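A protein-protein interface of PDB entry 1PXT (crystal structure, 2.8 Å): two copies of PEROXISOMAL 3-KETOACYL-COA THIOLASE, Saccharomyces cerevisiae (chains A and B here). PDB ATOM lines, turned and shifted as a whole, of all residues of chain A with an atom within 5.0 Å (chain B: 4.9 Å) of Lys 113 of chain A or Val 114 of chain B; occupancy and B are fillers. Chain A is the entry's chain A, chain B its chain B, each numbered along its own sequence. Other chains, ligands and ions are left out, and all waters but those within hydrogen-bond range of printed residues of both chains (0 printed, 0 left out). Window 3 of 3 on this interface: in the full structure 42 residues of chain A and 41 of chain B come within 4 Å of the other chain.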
ATOM      1  N   GLU A   7      21.562 -33.911 -20.188  1.00  0.00           N
ATOM      2  CA  GLU A   7      21.720 -32.824 -21.158  1.00  0.00           C
ATOM      3  C   GLU A   7      20.413 -32.486 -21.872  1.00  0.00           C
ATOM      4  O   GLU A   7      20.413 -31.696 -22.823  1.00  0.00           O
ATOM      5  CB  GLU A   7      22.736 -33.264 -22.231  1.00  0.00           C
ATOM      6  CG  GLU A   7      22.164 -34.339 -23.185  1.00  0.00           C
ATOM      7  CD  GLU A   7      23.221 -35.261 -23.768  1.00  0.00           C
ATOM      8  OE1 GLU A   7      24.237 -35.507 -23.082  1.00  0.00           O
ATOM      9  OE2 GLU A   7      23.015 -35.762 -24.901  1.00  0.00           O
ATOM     10  N   VAL A   9      16.619 -31.060 -22.662  1.00  0.00           N
ATOM     11  CA  VAL A   9      15.819 -29.848 -22.466  1.00  0.00           C
ATOM     12  C   VAL A   9      14.474 -30.450 -22.143  1.00  0.00           C
ATOM     13  O   VAL A   9      13.792 -31.036 -22.987  1.00  0.00           O
ATOM     14  CB  VAL A   9      15.704 -28.988 -23.742  1.00  0.00           C
ATOM     15  CG1 VAL A   9      14.939 -27.702 -23.434  1.00  0.00           C
ATOM     16  CG2 VAL A   9      17.092 -28.679 -24.291  1.00  0.00           C
ATOM     17  N   ALA A 109      15.128 -23.403 -25.696  1.00  0.00           N
ATOM     18  CA  ALA A 109      15.812 -24.677 -25.864  1.00  0.00           C
ATOM     19  C   ALA A 109      17.292 -24.417 -26.139  1.00  0.00           C
ATOM     20  O   ALA A 109      18.140 -24.738 -25.320  1.00  0.00           O
ATOM     21  CB  ALA A 109      15.188 -25.435 -27.018  1.00  0.00           C
ATOM     22  N   ASN A 110      17.570 -23.761 -27.261  1.00  0.00           N
ATOM     23  CA  ASN A 110      18.934 -23.441 -27.660  1.00  0.00           C
ATOM     24  C   ASN A 110      19.787 -22.824 -26.546  1.00  0.00           C
ATOM     25  O   ASN A 110      20.855 -23.333 -26.229  1.00  0.00           O
ATOM     26  CB  ASN A 110      18.925 -22.520 -28.879  1.00  0.00           C
ATOM     27  CG  ASN A 110      18.487 -23.237 -30.143  1.00  0.00           C
ATOM     28  OD1 ASN A 110      18.543 -24.451 -30.207  1.00  0.00           O
ATOM     29  ND2 ASN A 110      18.076 -22.491 -31.156  1.00  0.00           N
ATOM     30  N   LYS A 111      19.296 -21.778 -25.899  1.00  0.00           N
ATOM     31  CA  LYS A 111      20.078 -21.147 -24.842  1.00  0.00           C
ATOM     32  C   LYS A 111      20.457 -22.159 -23.773  1.00  0.00           C
ATOM     33  O   LYS A 111      21.557 -22.104 -23.198  1.00  0.00           O
ATOM     34  CB  LYS A 111      19.314 -19.963 -24.244  1.00  0.00           C
ATOM     35  CG  LYS A 111      18.985 -18.913 -25.277  1.00  0.00           C
ATOM     36  CD  LYS A 111      17.924 -17.933 -24.851  1.00  0.00           C
ATOM     37  CE  LYS A 111      18.146 -16.624 -25.601  1.00  0.00           C
ATOM     38  NZ  LYS A 111      17.002 -15.681 -25.607  1.00  0.00           N
ATOM     39  N   ILE A 112      19.546 -23.098 -23.519  1.00  0.00           N
ATOM     40  CA  ILE A 112      19.780 -24.144 -22.509  1.00  0.00           C
ATOM     41  C   ILE A 112      20.804 -25.179 -23.007  1.00  0.00           C
ATOM     42  O   ILE A 112      21.634 -25.669 -22.231  1.00  0.00           O
ATOM     43  CB  ILE A 112      18.429 -24.860 -22.085  1.00  0.00           C
ATOM     44  CG1 ILE A 112      17.429 -23.830 -21.559  1.00  0.00           C
ATOM     45  CG2 ILE A 112      18.691 -25.935 -21.001  1.00  0.00           C
ATOM     46  CD1 ILE A 112      16.116 -24.425 -21.158  1.00  0.00           C
ATOM     47  N   LYS A 113      20.721 -25.513 -24.292  1.00  0.00           N
ATOM     48  CA  LYS A 113      21.633 -26.480 -24.886  1.00  0.00           C
ATOM     49  C   LYS A 113      23.079 -25.936 -24.926  1.00  0.00           C
ATOM     50  O   LYS A 113      24.004 -26.539 -24.370  1.00  0.00           O
ATOM     51  CB  LYS A 113      21.107 -26.900 -26.263  1.00  0.00           C
ATOM     52  CG  LYS A 113      20.055 -28.020 -26.161  1.00  0.00           C
ATOM     53  CD  LYS A 113      19.032 -28.028 -27.288  1.00  0.00           C
ATOM     54  CE  LYS A 113      19.602 -28.496 -28.628  1.00  0.00           C
ATOM     55  NZ  LYS A 113      18.711 -28.135 -29.800  1.00  0.00           N
ATOM     56  N   VAL A 114      23.190 -24.699 -25.399  1.00  0.00           N
ATOM     57  CA  VAL A 114      24.430 -23.923 -25.549  1.00  0.00           C
ATOM     58  C   VAL A 114      24.941 -23.422 -24.187  1.00  0.00           C
ATOM     59  O   VAL A 114      25.807 -22.554 -24.116  1.00  0.00           O
ATOM     60  CB  VAL A 114      24.128 -22.747 -26.534  1.00  0.00           C
ATOM     61  CG1 VAL A 114      24.425 -21.413 -25.954  1.00  0.00           C
ATOM     62  CG2 VAL A 114      24.801 -22.956 -27.820  1.00  0.00           C
ATOM     63  N   GLY A 115      24.366 -23.951 -23.106  1.00  0.00           N
ATOM     64  CA  GLY A 115      24.763 -23.583 -21.753  1.00  0.00           C
ATOM     65  C   GLY A 115      24.459 -22.162 -21.316  1.00  0.00           C
ATOM     66  O   GLY A 115      24.678 -21.824 -20.145  1.00  0.00           O
ATOM     67  N   TYR A 275      11.873 -31.714 -25.169  1.00  0.00           N
ATOM     68  CA  TYR A 275      12.048 -31.018 -26.436  1.00  0.00           C
ATOM     69  C   TYR A 275      13.122 -31.811 -27.199  1.00  0.00           C
ATOM     70  O   TYR A 275      14.201 -32.073 -26.663  1.00  0.00           O
ATOM     71  CB  TYR A 275      12.531 -29.587 -26.156  1.00  0.00           C
ATOM     72  CG  TYR A 275      13.043 -28.863 -27.381  1.00  0.00           C
ATOM     73  CD1 TYR A 275      12.162 -28.267 -28.288  1.00  0.00           C
ATOM     74  CD2 TYR A 275      14.417 -28.798 -27.650  1.00  0.00           C
ATOM     75  CE1 TYR A 275      12.636 -27.632 -29.431  1.00  0.00           C
ATOM     76  CE2 TYR A 275      14.900 -28.163 -28.792  1.00  0.00           C
ATOM     77  CZ  TYR A 275      14.011 -27.587 -29.674  1.00  0.00           C
ATOM     78  OH  TYR A 275      14.502 -26.969 -30.794  1.00  0.00           O
ATOM     79  N   ILE A 276      12.814 -32.244 -28.412  1.00  0.00           N
ATOM     80  CA  ILE A 276      13.785 -33.010 -29.203  1.00  0.00           C
ATOM     81  C   ILE A 276      14.493 -32.106 -30.214  1.00  0.00           C
ATOM     82  O   ILE A 276      15.681 -31.826 -30.100  1.00  0.00           O
ATOM     83  CB  ILE A 276      13.101 -34.261 -29.912  1.00  0.00           C
ATOM     84  CG1 ILE A 276      12.887 -35.374 -28.908  1.00  0.00           C
ATOM     85  CG2 ILE A 276      13.974 -34.861 -30.987  1.00  0.00           C
ATOM     86  CD1 ILE A 276      14.133 -35.693 -28.134  1.00  0.00           C
ATOM     87  N   ASN B 110      23.916 -19.123 -31.534  1.00  0.00           N
ATOM     88  CA  ASN B 110      23.362 -20.331 -30.908  1.00  0.00           C
ATOM     89  C   ASN B 110      22.818 -21.375 -31.893  1.00  0.00           C
ATOM     90  O   ASN B 110      23.029 -22.582 -31.697  1.00  0.00           O
ATOM     91  CB  ASN B 110      22.245 -19.946 -29.924  1.00  0.00           C
ATOM     92  CG  ASN B 110      22.776 -19.547 -28.550  1.00  0.00           C
ATOM     93  OD1 ASN B 110      23.949 -19.761 -28.246  1.00  0.00           O
ATOM     94  ND2 ASN B 110      21.913 -18.962 -27.715  1.00  0.00           N
ATOM     95  N   LYS B 111      22.120 -20.935 -32.938  1.00  0.00           N
ATOM     96  CA  LYS B 111      21.555 -21.883 -33.889  1.00  0.00           C
ATOM     97  C   LYS B 111      22.648 -22.676 -34.569  1.00  0.00           C
ATOM     98  O   LYS B 111      22.592 -23.914 -34.665  1.00  0.00           O
ATOM     99  CB  LYS B 111      20.684 -21.172 -34.924  1.00  0.00           C
ATOM    100  CG  LYS B 111      19.371 -20.700 -34.390  1.00  0.00           C
ATOM    101  CD  LYS B 111      18.561 -19.854 -35.392  1.00  0.00           C
ATOM    102  CE  LYS B 111      17.241 -19.414 -34.723  1.00  0.00           C
ATOM    103  NZ  LYS B 111      16.537 -18.196 -35.259  1.00  0.00           N
ATOM    104  N   ILE B 112      23.639 -21.936 -35.060  1.00  0.00           N
ATOM    105  CA  ILE B 112      24.819 -22.500 -35.734  1.00  0.00           C
ATOM    106  C   ILE B 112      25.485 -23.454 -34.748  1.00  0.00           C
ATOM    107  O   ILE B 112      25.761 -24.608 -35.064  1.00  0.00           O
ATOM    108  CB  ILE B 112      25.881 -21.395 -36.039  1.00  0.00           C
ATOM    109  CG1 ILE B 112      25.441 -20.458 -37.172  1.00  0.00           C
ATOM    110  CG2 ILE B 112      27.185 -22.029 -36.366  1.00  0.00           C
ATOM    111  CD1 ILE B 112      26.348 -19.216 -37.313  1.00  0.00           C
ATOM    112  N   LYS B 113      25.703 -22.942 -33.541  1.00  0.00           N
ATOM    113  CA  LYS B 113      26.364 -23.679 -32.490  1.00  0.00           C
ATOM    114  C   LYS B 113      25.705 -24.953 -32.248  1.00  0.00           C
ATOM    115  O   LYS B 113      26.355 -25.960 -32.115  1.00  0.00           O
ATOM    116  CB  LYS B 113      26.359 -22.915 -31.185  1.00  0.00           C
ATOM    117  CG  LYS B 113      27.255 -21.734 -31.211  1.00  0.00           C
ATOM    118  CD  LYS B 113      27.129 -20.919 -29.974  1.00  0.00           C
ATOM    119  CE  LYS B 113      27.942 -21.487 -28.859  1.00  0.00           C
ATOM    120  NZ  LYS B 113      28.026 -20.445 -27.806  1.00  0.00           N
ATOM    121  N   VAL B 114      24.391 -24.903 -32.180  1.00  0.00           N
ATOM    122  CA  VAL B 114      23.593 -26.073 -31.881  1.00  0.00           C
ATOM    123  C   VAL B 114      23.372 -26.929 -33.125  1.00  0.00           C
ATOM    124  O   VAL B 114      22.828 -28.005 -33.047  1.00  0.00           O
ATOM    125  CB  VAL B 114      22.263 -25.642 -31.191  1.00  0.00           C
ATOM    126  CG1 VAL B 114      21.148 -25.489 -32.188  1.00  0.00           C
ATOM    127  CG2 VAL B 114      21.939 -26.564 -30.118  1.00  0.00           C
ATOM    128  N   GLY B 115      23.814 -26.483 -34.281  1.00  0.00           N
ATOM    129  CA  GLY B 115      23.616 -27.327 -35.427  1.00  0.00           C
ATOM    130  C   GLY B 115      22.339 -27.077 -36.161  1.00  0.00           C
ATOM    131  O   GLY B 115      22.122 -27.647 -37.233  1.00  0.00           O
ATOM    132  N   GLN B 116      21.508 -26.182 -35.646  1.00  0.00           N
ATOM    133  CA  GLN B 116      20.245 -25.911 -36.318  1.00  0.00           C
ATOM    134  C   GLN B 116      20.539 -25.383 -37.715  1.00  0.00           C
ATOM    135  O   GLN B 116      19.872 -25.768 -38.670  1.00  0.00           O
ATOM    136  CB  GLN B 116      19.426 -24.924 -35.508  1.00  0.00           C
ATOM    137  CG  GLN B 116      18.046 -24.608 -36.050  1.00  0.00           C
ATOM    138  CD  GLN B 116      17.292 -23.747 -35.066  1.00  0.00           C
ATOM    139  OE1 GLN B 116      17.429 -23.923 -33.842  1.00  0.00           O
ATOM    140  NE2 GLN B 116      16.537 -22.784 -35.572  1.00  0.00           N
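The side-chain amide oxygen of Gln 116 of chain B is in hydrogen-bond range of the side-chain amide nitrogen of Asn 110 of chain A.
O of Lys 111 of chain B lies within hydrogen-bond range of N of Gln 116 of chain B (2.7 Å).
Among the printed residues, merely in contact across the chains: Asn 110 of chain A with Lys 111 of chain B (3.9 Å), Asn 110 of chain A with Val 114 of chain B (3.4 Å), Lys 111 of chain A with Asn 110 of chain B (3.8 Å), Lys 113 of chain A with Val 114 of chain B (3.4 Å), Val 114 of chain A with Asn 110 of chain B (2.9 Å) and Val 114 of chain A with Lys 113 of chain B (3.6 Å).
Lys 113 of chain A touches just one residue of chain B: Val 114 (3.4 Å). Of chain A, only Asn 110 (3.4 Å) and Lys 113 (3.4 Å) come within 4 Å of Val 114 of chain B. Of the printed residues of chain A, Lys 111 of chain B touches Asn 110. Of the printed residues of chain A, Asn 110 of chain B touches Lys 111 (3.8 Å) and Val 114 (2.9 Å). Printed residues of chain A within 4 Å of Gln 116 of chain B: Asn 110 (3.1 Å). Of the printed residues of chain B, Val 114 of chain A touches Asn 110 (2.9 Å) and Lys 113 (3.6 Å). Of the printed residues of chain B, Asn 110 of chain A touches Lys 111 (3.9 Å), Val 114 (3.4 Å) and Gln 116 (3.1 Å). Val 9 of chain A touches none of the printed residues of chain B. Glu 7 of chain A touches none of the printed residues of chain B. The nearest printed residue of chain B that does not touch Lys 113 of chain A is Gln 116 of chain B (6.0 Å).
Hydrophobic or aromatic side chains of chain A that line the printed part of chain B: Val 114. Along chain B the printed residues that touch a printed residue of chain A span positions 110 to 116.
Asn 110 of chain A touches Lys 111 of chain B, and with the chains exchanged Lys 111 of chain A touches Asn 110 of chain B. Asn 110 of chain A touches Val 114 of chain B, and with the chains exchanged Val 114 of chain A touches Asn 110 of chain B. Lys 113 of chain A touches Val 114 of chain B, and with the chains exchanged Val 114 of chain A touches Lys 113 of chain B. Of the 7 pairs that touch across the chains among the printed residues, 6 have their exchanged pair printed and touching as well.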
